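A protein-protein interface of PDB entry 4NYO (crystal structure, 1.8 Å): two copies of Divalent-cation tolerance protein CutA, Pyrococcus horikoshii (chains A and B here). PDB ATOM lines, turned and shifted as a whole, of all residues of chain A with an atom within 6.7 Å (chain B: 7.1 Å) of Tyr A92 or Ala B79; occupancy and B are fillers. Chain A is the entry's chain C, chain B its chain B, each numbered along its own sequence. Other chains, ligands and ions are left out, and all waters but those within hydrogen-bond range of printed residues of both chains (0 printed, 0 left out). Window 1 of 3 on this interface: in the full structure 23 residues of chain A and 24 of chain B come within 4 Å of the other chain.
No position is printed for both chains.
Of the printed residues of chain B, Asn A89 touches Lys B70 (3.95 Å), Pro B78 (2.8 Å), Ala B79 (3.9 Å) and Ile B80 (2.9 Å). Tyr A92 touches just these residues of chain B: Val B77, Pro B78 and Ala B79. Printed residues of chain A within 4 Å of Tyr B39: Ala A28 and CSD A29. Tyr B75 touches none of the printed residues of chain A. Printed residues of chain A within 4 Å of Val B77: Asp A91 (3.9 Å) and Tyr A92 (3.9 Å). Ala B79 touches just these residues of chain A: Asn A89 and Tyr A92. Printed residues of chain A within 4 Å of Ile B80: Val A88 and Asn A89.
Printed residues of chain B that touch a printed residue of chain A: Tyr B39, Lys B70, Val B77, Pro B78, Ala B79 and Ile B80. Printed residues of chain A that touch a printed residue of chain B: Ala A28, CSD A29, Val A88, Asn A89, Asp A91 and Tyr A92. Hydrophobic or aromatic side chains of chain A that line the printed part of chain B: Val A88 and Tyr A92. Among the printed residues, 12 pairs touch across the chains. Among the printed residues, Asp or Glu carboxylates within 4 Å of a Lys or Arg side-chain nitrogen of the other chain: Asp A91 with Lys B70 (3.0 Å).
NZ of Lys B70 is in salt-bridge range of OD1 of Asp A91 (3.0 Å). ND2 of Asn A89 is in hydrogen-bond range of O of Pro B78 (2.8 Å). The side-chain amide oxygen (OD1) of Asn A89 sits at hydrogen-bond distance from the backbone NH (N) of Ile B80 (2.9 Å).
Among the printed residues, merely in contact across the chains: Ala A28 with Tyr B39, CSD A29 with Tyr B39, Val A88 with Ile B80, Asn A89 with Lys B70, Asn A89 with Ala B79, Asp A91 with Val B77, Tyr A92 with Val B77, Tyr A92 with Pro B78 and Tyr A92 with Ala B79.
The side-chain amide nitrogen of Asn A89 sits at hydrogen-bond distance from the side-chain carboxylate of Asp A91, 2.9 Å away. The side-chain amino group of Lys A56 sits close to OD2 of CSD A29, 3.6 Å away. OD1 of CSD A29 lies within hydrogen-bond range of the side-chain hydroxyl (OH) of Tyr A92. O of Ala B79 lies within hydrogen-bond range of OG1 of Thr B6, at 2.7 Å. N of Ala A28 is in hydrogen-bond range of O of Lys A56, at 3.0 Å.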
ATOM      1  N   MET A   1     -18.801  -3.596   7.941  1.00  0.00           N
ATOM      2  CA  MET A   1     -18.230  -2.848   6.787  1.00  0.00           C
ATOM      3  C   MET A   1     -17.180  -1.862   7.276  1.00  0.00           C
ATOM      4  O   MET A   1     -17.015  -1.654   8.484  1.00  0.00           O
ATOM      5  CB  MET A   1     -19.331  -2.089   6.027  1.00  0.00           C
ATOM      6  CG  MET A   1     -19.937  -0.905   6.776  1.00  0.00           C
ATOM      7  SD  MET A   1     -21.033   0.109   5.735  1.00  0.00           S
ATOM      8  CE  MET A   1     -19.835   1.071   4.813  1.00  0.00           C
ATOM      9  N   ALA A  28     -18.145  -0.636  -2.988  1.00  0.00           N
ATOM     10  CA  ALA A  28     -19.524  -0.493  -3.446  1.00  0.00           C
ATOM     11  C   ALA A  28     -19.749   0.939  -3.919  1.00  0.00           C
ATOM     12  O   ALA A  28     -20.607   1.208  -4.765  1.00  0.00           O
ATOM     13  CB  ALA A  28     -20.498  -0.846  -2.326  1.00  0.00           C
ATOM     14  N   CSD A  29     -18.987   1.864  -3.348  1.00  0.00           N
ATOM     15  CA  CSD A  29     -19.072   3.244  -3.772  1.00  0.00           C
ATOM     16  CB  CSD A  29     -20.501   3.756  -3.645  1.00  0.00           C
ATOM     17  SG  CSD A  29     -21.030   4.287  -2.054  1.00  0.00           S
ATOM     18  C   CSD A  29     -18.087   4.169  -3.081  1.00  0.00           C
ATOM     19  O   CSD A  29     -17.378   3.773  -2.156  1.00  0.00           O
ATOM     20  OD1 CSD A  29     -20.282   3.525  -1.060  1.00  0.00           O
ATOM     21  OD2 CSD A  29     -20.838   5.733  -2.045  1.00  0.00           O
ATOM     22  N   LYS A  56     -16.337   2.929   0.518  1.00  0.00           N
ATOM     23  CA  LYS A  56     -17.114   2.048   1.382  1.00  0.00           C
ATOM     24  C   LYS A  56     -17.083   0.612   0.857  1.00  0.00           C
ATOM     25  O   LYS A  56     -17.409   0.360  -0.308  1.00  0.00           O
ATOM     26  CB  LYS A  56     -18.552   2.563   1.464  1.00  0.00           C
ATOM     27  CG  LYS A  56     -18.619   4.078   1.638  1.00  0.00           C
ATOM     28  CD  LYS A  56     -20.043   4.616   1.632  1.00  0.00           C
ATOM     29  CE  LYS A  56     -20.045   6.064   1.155  1.00  0.00           C
ATOM     30  NZ  LYS A  56     -21.347   6.757   1.398  1.00  0.00           N
ATOM     31  N   VAL A  88     -24.574   0.231  11.005  1.00  0.00           N
ATOM     32  CA  VAL A  88     -25.102   0.860   9.803  1.00  0.00           C
ATOM     33  C   VAL A  88     -26.478   0.258   9.524  1.00  0.00           C
ATOM     34  O   VAL A  88     -26.750  -0.877   9.940  1.00  0.00           O
ATOM     35  CB  VAL A  88     -24.141   0.594   8.613  1.00  0.00           C
ATOM     36  CG1 VAL A  88     -23.852  -0.897   8.507  1.00  0.00           C
ATOM     37  CG2 VAL A  88     -24.739   1.123   7.310  1.00  0.00           C
ATOM     38  N   ASN A  89     -27.362   1.005   8.859  1.00  0.00           N
ATOM     39  CA  ASN A  89     -28.678   0.441   8.553  1.00  0.00           C
ATOM     40  C   ASN A  89     -28.409  -0.813   7.730  1.00  0.00           C
ATOM     41  O   ASN A  89     -27.581  -0.813   6.814  1.00  0.00           O
ATOM     42  CB  ASN A  89     -29.580   1.450   7.817  1.00  0.00           C
ATOM     43  CG  ASN A  89     -28.911   2.094   6.628  1.00  0.00           C
ATOM     44  OD1 ASN A  89     -27.782   2.574   6.718  1.00  0.00           O
ATOM     45  ND2 ASN A  89     -29.619   2.134   5.506  1.00  0.00           N
ATOM     46  N   GLU A  90     -29.107  -1.891   8.070  1.00  0.00           N
ATOM     47  CA  GLU A  90     -28.860  -3.176   7.444  1.00  0.00           C
ATOM     48  C   GLU A  90     -29.351  -3.397   6.022  1.00  0.00           C
ATOM     49  O   GLU A  90     -28.951  -4.364   5.374  1.00  0.00           O
ATOM     50  CB  GLU A  90     -29.330  -4.266   8.417  1.00  0.00           C
ATOM     51  CG  GLU A  90     -28.789  -3.952   9.830  1.00  0.00           C
ATOM     52  CD  GLU A  90     -28.992  -5.047  10.859  1.00  0.00           C
ATOM     53  OE1 GLU A  90     -30.069  -5.675  10.867  1.00  0.00           O
ATOM     54  OE2 GLU A  90     -28.068  -5.258  11.683  1.00  0.00           O
ATOM     55  N   ASP A  91     -30.192  -2.502   5.518  1.00  0.00           N
ATOM     56  CA  ASP A  91     -30.639  -2.639   4.137  1.00  0.00           C
ATOM     57  C   ASP A  91     -29.509  -2.098   3.254  1.00  0.00           C
ATOM     58  O   ASP A  91     -29.285  -2.581   2.144  1.00  0.00           O
ATOM     59  CB  ASP A  91     -31.953  -1.879   3.898  1.00  0.00           C
ATOM     60  CG  ASP A  91     -31.912  -0.452   4.394  1.00  0.00           C
ATOM     61  OD1 ASP A  91     -31.394  -0.215   5.504  1.00  0.00           O
ATOM     62  OD2 ASP A  91     -32.419   0.435   3.677  1.00  0.00           O
ATOM     63  N   TYR A  92     -28.780  -1.113   3.772  1.00  0.00           N
ATOM     64  CA  TYR A  92     -27.652  -0.534   3.048  1.00  0.00           C
ATOM     65  C   TYR A  92     -26.499  -1.535   3.071  1.00  0.00           C
ATOM     66  O   TYR A  92     -25.802  -1.724   2.079  1.00  0.00           O
ATOM     67  CB  TYR A  92     -27.221   0.786   3.698  1.00  0.00           C
ATOM     68  CG  TYR A  92     -25.994   1.406   3.064  1.00  0.00           C
ATOM     69  CD1 TYR A  92     -24.715   1.085   3.517  1.00  0.00           C
ATOM     70  CD2 TYR A  92     -26.113   2.281   1.983  1.00  0.00           C
ATOM     71  CE1 TYR A  92     -23.582   1.615   2.907  1.00  0.00           C
ATOM     72  CE2 TYR A  92     -24.983   2.816   1.364  1.00  0.00           C
ATOM     73  CZ  TYR A  92     -23.721   2.476   1.834  1.00  0.00           C
ATOM     74  OH  TYR A  92     -22.593   2.992   1.232  1.00  0.00           O
ATOM     75  N   LEU A  93     -26.309  -2.192   4.211  1.00  0.00           N
ATOM     76  CA  LEU A  93     -25.244  -3.176   4.332  1.00  0.00           C
ATOM     77  C   LEU A  93     -25.503  -4.368   3.416  1.00  0.00           C
ATOM     78  O   LEU A  93     -24.570  -4.931   2.846  1.00  0.00           O
ATOM     79  CB  LEU A  93     -25.117  -3.644   5.786  1.00  0.00           C
ATOM     80  CG  LEU A  93     -23.925  -4.553   6.095  1.00  0.00           C
ATOM     81  CD1 LEU A  93     -22.641  -3.944   5.570  1.00  0.00           C
ATOM     82  CD2 LEU A  93     -23.838  -4.748   7.600  1.00  0.00           C
ATOM     83  N   LYS A  94     -26.770  -4.751   3.265  1.00  0.00           N
ATOM     84  CA  LYS A  94     -27.101  -5.880   2.395  1.00  0.00           C
ATOM     85  C   LYS A  94     -26.739  -5.507   0.961  1.00  0.00           C
ATOM     86  O   LYS A  94     -26.163  -6.307   0.222  1.00  0.00           O
ATOM     87  CB  LYS A  94     -28.595  -6.224   2.496  1.00  0.00           C
ATOM     88  CG  LYS A  94     -29.036  -7.432   1.637  1.00  0.00           C
ATOM     89  CD  LYS A  94     -28.311  -8.728   2.017  1.00  0.00           C
ATOM     90  CE  LYS A  94     -28.783  -9.899   1.146  1.00  0.00           C
ATOM     91  NZ  LYS A  94     -28.126 -11.204   1.474  1.00  0.00           N
ATOM     92  N   TRP A  95     -27.091  -4.285   0.574  1.00  0.00           N
ATOM     93  CA  TRP A  95     -26.789  -3.782  -0.761  1.00  0.00           C
ATOM     94  C   TRP A  95     -25.286  -3.792  -1.001  1.00  0.00           C
ATOM     95  O   TRP A  95     -24.810  -4.277  -2.030  1.00  0.00           O
ATOM     96  CB  TRP A  95     -27.297  -2.345  -0.914  1.00  0.00           C
ATOM     97  CG  TRP A  95     -26.693  -1.614  -2.086  1.00  0.00           C
ATOM     98  CD1 TRP A  95     -27.037  -1.744  -3.405  1.00  0.00           C
ATOM     99  CD2 TRP A  95     -25.619  -0.665  -2.043  1.00  0.00           C
ATOM    100  NE1 TRP A  95     -26.242  -0.931  -4.185  1.00  0.00           N
ATOM    101  CE2 TRP A  95     -25.364  -0.259  -3.373  1.00  0.00           C
ATOM    102  CE3 TRP A  95     -24.845  -0.119  -1.008  1.00  0.00           C
ATOM    103  CZ2 TRP A  95     -24.364   0.668  -3.696  1.00  0.00           C
ATOM    104  CZ3 TRP A  95     -23.848   0.806  -1.329  1.00  0.00           C
ATOM    105  CH2 TRP A  95     -23.620   1.189  -2.663  1.00  0.00           C
ATOM    106  N   LEU A  96     -24.544  -3.245  -0.041  1.00  0.00           N
ATOM    107  CA  LEU A  96     -23.094  -3.157  -0.137  1.00  0.00           C
ATOM    108  C   LEU A  96     -22.398  -4.503  -0.311  1.00  0.00           C
ATOM    109  O   LEU A  96     -21.513  -4.635  -1.154  1.00  0.00           O
ATOM    110  CB  LEU A  96     -22.533  -2.426   1.093  1.00  0.00           C
ATOM    111  CG  LEU A  96     -21.013  -2.255   1.185  1.00  0.00           C
ATOM    112  CD1 LEU A  96     -20.690  -0.943   1.880  1.00  0.00           C
ATOM    113  CD2 LEU A  96     -20.396  -3.435   1.933  1.00  0.00           C
ATOM    114  N   ILE A  97     -22.788  -5.502   0.475  1.00  0.00           N
ATOM    115  CA  ILE A  97     -22.152  -6.806   0.347  1.00  0.00           C
ATOM    116  C   ILE A  97     -22.513  -7.518  -0.957  1.00  0.00           C
ATOM    117  O   ILE A  97     -21.714  -8.282  -1.481  1.00  0.00           O
ATOM    118  CB  ILE A  97     -22.480  -7.735   1.550  1.00  0.00           C
ATOM    119  CG1 ILE A  97     -23.965  -8.083   1.579  1.00  0.00           C
ATOM    120  CG2 ILE A  97     -22.072  -7.055   2.849  1.00  0.00           C
ATOM    121  CD1 ILE A  97     -24.301  -9.178   2.578  1.00  0.00           C
ATOM    122  N   VAL B   4     -22.541  10.124  12.982  1.00  0.00           N
ATOM    123  CA  VAL B   4     -23.341   9.392  12.009  1.00  0.00           C
ATOM    124  C   VAL B   4     -23.217  10.090  10.664  1.00  0.00           C
ATOM    125  O   VAL B   4     -23.461  11.295  10.549  1.00  0.00           O
ATOM    126  CB  VAL B   4     -24.829   9.312  12.412  1.00  0.00           C
ATOM    127  CG1 VAL B   4     -25.635   8.680  11.278  1.00  0.00           C
ATOM    128  CG2 VAL B   4     -24.981   8.469  13.674  1.00  0.00           C
ATOM    129  N   TYR B   5     -22.831   9.324   9.650  1.00  0.00           N
ATOM    130  CA  TYR B   5     -22.650   9.852   8.307  1.00  0.00           C
ATOM    131  C   TYR B   5     -23.727   9.359   7.348  1.00  0.00           C
ATOM    132  O   TYR B   5     -23.976   8.162   7.250  1.00  0.00           O
ATOM    133  CB  TYR B   5     -21.272   9.447   7.776  1.00  0.00           C
ATOM    134  CG  TYR B   5     -20.939  10.008   6.408  1.00  0.00           C
ATOM    135  CD1 TYR B   5     -20.766   9.166   5.309  1.00  0.00           C
ATOM    136  CD2 TYR B   5     -20.780  11.380   6.219  1.00  0.00           C
ATOM    137  CE1 TYR B   5     -20.440   9.678   4.052  1.00  0.00           C
ATOM    138  CE2 TYR B   5     -20.453  11.904   4.968  1.00  0.00           C
ATOM    139  CZ  TYR B   5     -20.284  11.046   3.890  1.00  0.00           C
ATOM    140  OH  TYR B   5     -19.945  11.565   2.661  1.00  0.00           O
ATOM    141  N   THR B   6     -24.363  10.293   6.649  1.00  0.00           N
ATOM    142  CA  THR B   6     -25.394   9.945   5.676  1.00  0.00           C
ATOM    143  C   THR B   6     -25.255  10.904   4.502  1.00  0.00           C
ATOM    144  O   THR B   6     -24.569  11.918   4.613  1.00  0.00           O
ATOM    145  CB  THR B   6     -26.816  10.066   6.284  1.00  0.00           C
ATOM    146  OG1 THR B   6     -27.784   9.632   5.320  1.00  0.00           O
ATOM    147  CG2 THR B   6     -27.112  11.513   6.677  1.00  0.00           C
ATOM    148  N   THR B   7     -25.878  10.583   3.371  1.00  0.00           N
ATOM    149  CA  THR B   7     -25.783  11.466   2.218  1.00  0.00           C
ATOM    150  C   THR B   7     -27.161  11.763   1.655  1.00  0.00           C
ATOM    151  O   THR B   7     -28.076  10.948   1.772  1.00  0.00           O
ATOM    152  CB  THR B   7     -24.907  10.858   1.109  1.00  0.00           C
ATOM    153  OG1 THR B   7     -25.586   9.751   0.508  1.00  0.00           O
ATOM    154  CG2 THR B   7     -23.581  10.386   1.685  1.00  0.00           C
ATOM    155  N   TYR B  39     -21.173   5.056  -7.411  1.00  0.00           N
ATOM    156  CA  TYR B  39     -21.644   3.840  -6.768  1.00  0.00           C
ATOM    157  C   TYR B  39     -22.313   2.863  -7.719  1.00  0.00           C
ATOM    158  O   TYR B  39     -22.771   3.232  -8.803  1.00  0.00           O
ATOM    159  CB  TYR B  39     -22.640   4.192  -5.661  1.00  0.00           C
ATOM    160  CG  TYR B  39     -23.829   4.985  -6.144  1.00  0.00           C
ATOM    161  CD1 TYR B  39     -23.713   6.341  -6.434  1.00  0.00           C
ATOM    162  CD2 TYR B  39     -25.065   4.371  -6.344  1.00  0.00           C
ATOM    163  CE1 TYR B  39     -24.800   7.072  -6.912  1.00  0.00           C
ATOM    164  CE2 TYR B  39     -26.159   5.090  -6.823  1.00  0.00           C
ATOM    165  CZ  TYR B  39     -26.017   6.440  -7.105  1.00  0.00           C
ATOM    166  OH  TYR B  39     -27.091   7.160  -7.581  1.00  0.00           O
ATOM    167  N   ALA B  53     -23.602  14.510   5.080  1.00  0.00           N
ATOM    168  CA  ALA B  53     -23.908  15.067   6.386  1.00  0.00           C
ATOM    169  C   ALA B  53     -23.267  14.287   7.519  1.00  0.00           C
ATOM    170  O   ALA B  53     -23.406  13.068   7.607  1.00  0.00           O
ATOM    171  CB  ALA B  53     -25.419  15.125   6.583  1.00  0.00           C
ATOM    172  N   ILE B  69     -34.213   8.807  10.560  1.00  0.00           N
ATOM    173  CA  ILE B  69     -33.611   9.154   9.285  1.00  0.00           C
ATOM    174  C   ILE B  69     -34.250   8.300   8.191  1.00  0.00           C
ATOM    175  O   ILE B  69     -34.521   8.787   7.094  1.00  0.00           O
ATOM    176  CB  ILE B  69     -32.081   8.935   9.304  1.00  0.00           C
ATOM    177  CG1 ILE B  69     -31.423   9.923  10.277  1.00  0.00           C
ATOM    178  CG2 ILE B  69     -31.509   9.129   7.905  1.00  0.00           C
ATOM    179  CD1 ILE B  69     -29.920   9.706  10.475  1.00  0.00           C
ATOM    180  N   LYS B  70     -34.501   7.030   8.500  1.00  0.00           N
ATOM    181  CA  LYS B  70     -35.126   6.114   7.542  1.00  0.00           C
ATOM    182  C   LYS B  70     -36.491   6.622   7.087  1.00  0.00           C
ATOM    183  O   LYS B  70     -36.827   6.555   5.905  1.00  0.00           O
ATOM    184  CB  LYS B  70     -35.309   4.727   8.165  1.00  0.00           C
ATOM    185  CG  LYS B  70     -34.139   3.778   8.006  1.00  0.00           C
ATOM    186  CD  LYS B  70     -34.427   2.477   8.747  1.00  0.00           C
ATOM    187  CE  LYS B  70     -33.497   1.355   8.324  1.00  0.00           C
ATOM    188  NZ  LYS B  70     -33.761   0.867   6.937  1.00  0.00           N
ATOM    189  N   HIS B  73     -35.713  10.211   5.103  1.00  0.00           N
ATOM    190  CA  HIS B  73     -34.828  10.215   3.948  1.00  0.00           C
ATOM    191  C   HIS B  73     -35.461  10.015   2.573  1.00  0.00           C
ATOM    192  O   HIS B  73     -36.274   9.115   2.369  1.00  0.00           O
ATOM    193  CB  HIS B  73     -33.710   9.186   4.150  1.00  0.00           C
ATOM    194  CG  HIS B  73     -32.407   9.596   3.539  1.00  0.00           C
ATOM    195  ND1 HIS B  73     -32.239   9.755   2.180  1.00  0.00           N
ATOM    196  CD2 HIS B  73     -31.223   9.925   4.107  1.00  0.00           C
ATOM    197  CE1 HIS B  73     -31.009  10.168   1.938  1.00  0.00           C
ATOM    198  NE2 HIS B  73     -30.372  10.281   3.090  1.00  0.00           N
ATOM    199  N   TYR B  75     -33.955   9.009  -0.122  1.00  0.00           N
ATOM    200  CA  TYR B  75     -33.428   7.787  -0.736  1.00  0.00           C
ATOM    201  C   TYR B  75     -34.154   6.582  -0.151  1.00  0.00           C
ATOM    202  O   TYR B  75     -34.462   6.563   1.037  1.00  0.00           O
ATOM    203  CB  TYR B  75     -31.931   7.613  -0.451  1.00  0.00           C
ATOM    204  CG  TYR B  75     -30.990   8.509  -1.225  1.00  0.00           C
ATOM    205  CD1 TYR B  75     -31.347   9.045  -2.463  1.00  0.00           C
ATOM    206  CD2 TYR B  75     -29.705   8.763  -0.747  1.00  0.00           C
ATOM    207  CE1 TYR B  75     -30.440   9.811  -3.208  1.00  0.00           C
ATOM    208  CE2 TYR B  75     -28.792   9.525  -1.481  1.00  0.00           C
ATOM    209  CZ  TYR B  75     -29.165  10.043  -2.708  1.00  0.00           C
ATOM    210  OH  TYR B  75     -28.256  10.779  -3.434  1.00  0.00           O
ATOM    211  N   VAL B  77     -32.858   3.525  -0.105  1.00  0.00           N
ATOM    212  CA  VAL B  77     -31.798   2.798   0.587  1.00  0.00           C
ATOM    213  C   VAL B  77     -30.667   3.785   0.882  1.00  0.00           C
ATOM    214  O   VAL B  77     -29.643   3.806   0.201  1.00  0.00           O
ATOM    215  CB  VAL B  77     -31.250   1.635  -0.274  1.00  0.00           C
ATOM    216  CG1 VAL B  77     -30.184   0.873   0.499  1.00  0.00           C
ATOM    217  CG2 VAL B  77     -32.382   0.696  -0.667  1.00  0.00           C
ATOM    218  N   PRO B  78     -30.851   4.631   1.906  1.00  0.00           N
ATOM    219  CA  PRO B  78     -29.839   5.621   2.280  1.00  0.00           C
ATOM    220  C   PRO B  78     -28.672   5.007   3.043  1.00  0.00           C
ATOM    221  O   PRO B  78     -28.754   3.877   3.516  1.00  0.00           O
ATOM    222  CB  PRO B  78     -30.621   6.584   3.155  1.00  0.00           C
ATOM    223  CG  PRO B  78     -31.538   5.658   3.892  1.00  0.00           C
ATOM    224  CD  PRO B  78     -32.028   4.728   2.787  1.00  0.00           C
ATOM    225  N   ALA B  79     -27.591   5.768   3.158  1.00  0.00           N
ATOM    226  CA  ALA B  79     -26.421   5.326   3.904  1.00  0.00           C
ATOM    227  C   ALA B  79     -26.536   5.970   5.279  1.00  0.00           C
ATOM    228  O   ALA B  79     -26.608   7.192   5.384  1.00  0.00           O
ATOM    229  CB  ALA B  79     -25.146   5.791   3.217  1.00  0.00           C
ATOM    230  N   ILE B  80     -26.596   5.151   6.324  1.00  0.00           N
ATOM    231  CA  ILE B  80     -26.671   5.656   7.693  1.00  0.00           C
ATOM    232  C   ILE B  80     -25.575   4.914   8.450  1.00  0.00           C
ATOM    233  O   ILE B  80     -25.803   3.867   9.070  1.00  0.00           O
ATOM    234  CB  ILE B  80     -28.041   5.375   8.328  1.00  0.00           C
ATOM    235  CG1 ILE B  80     -29.154   5.856   7.393  1.00  0.00           C
ATOM    236  CG2 ILE B  80     -28.139   6.096   9.674  1.00  0.00           C
ATOM    237  CD1 ILE B  80     -30.562   5.543   7.894  1.00  0.00           C
ATOM    238  N   ILE B  81     -24.384   5.495   8.386  1.00  0.00           N
ATOM    239  CA  ILE B  81     -23.173   4.934   8.963  1.00  0.00           C
ATOM    240  C   ILE B  81     -22.781   5.499  10.322  1.00  0.00           C
ATOM    241  O   ILE B  81     -22.576   6.702  10.472  1.00  0.00           O
ATOM    242  CB  ILE B  81     -22.024   5.141   7.961  1.00  0.00           C
ATOM    243  CG1 ILE B  81     -22.372   4.422   6.652  1.00  0.00           C
ATOM    244  CG2 ILE B  81     -20.717   4.655   8.540  1.00  0.00           C
ATOM    245  CD1 ILE B  81     -21.468   4.779   5.478  1.00  0.00           C
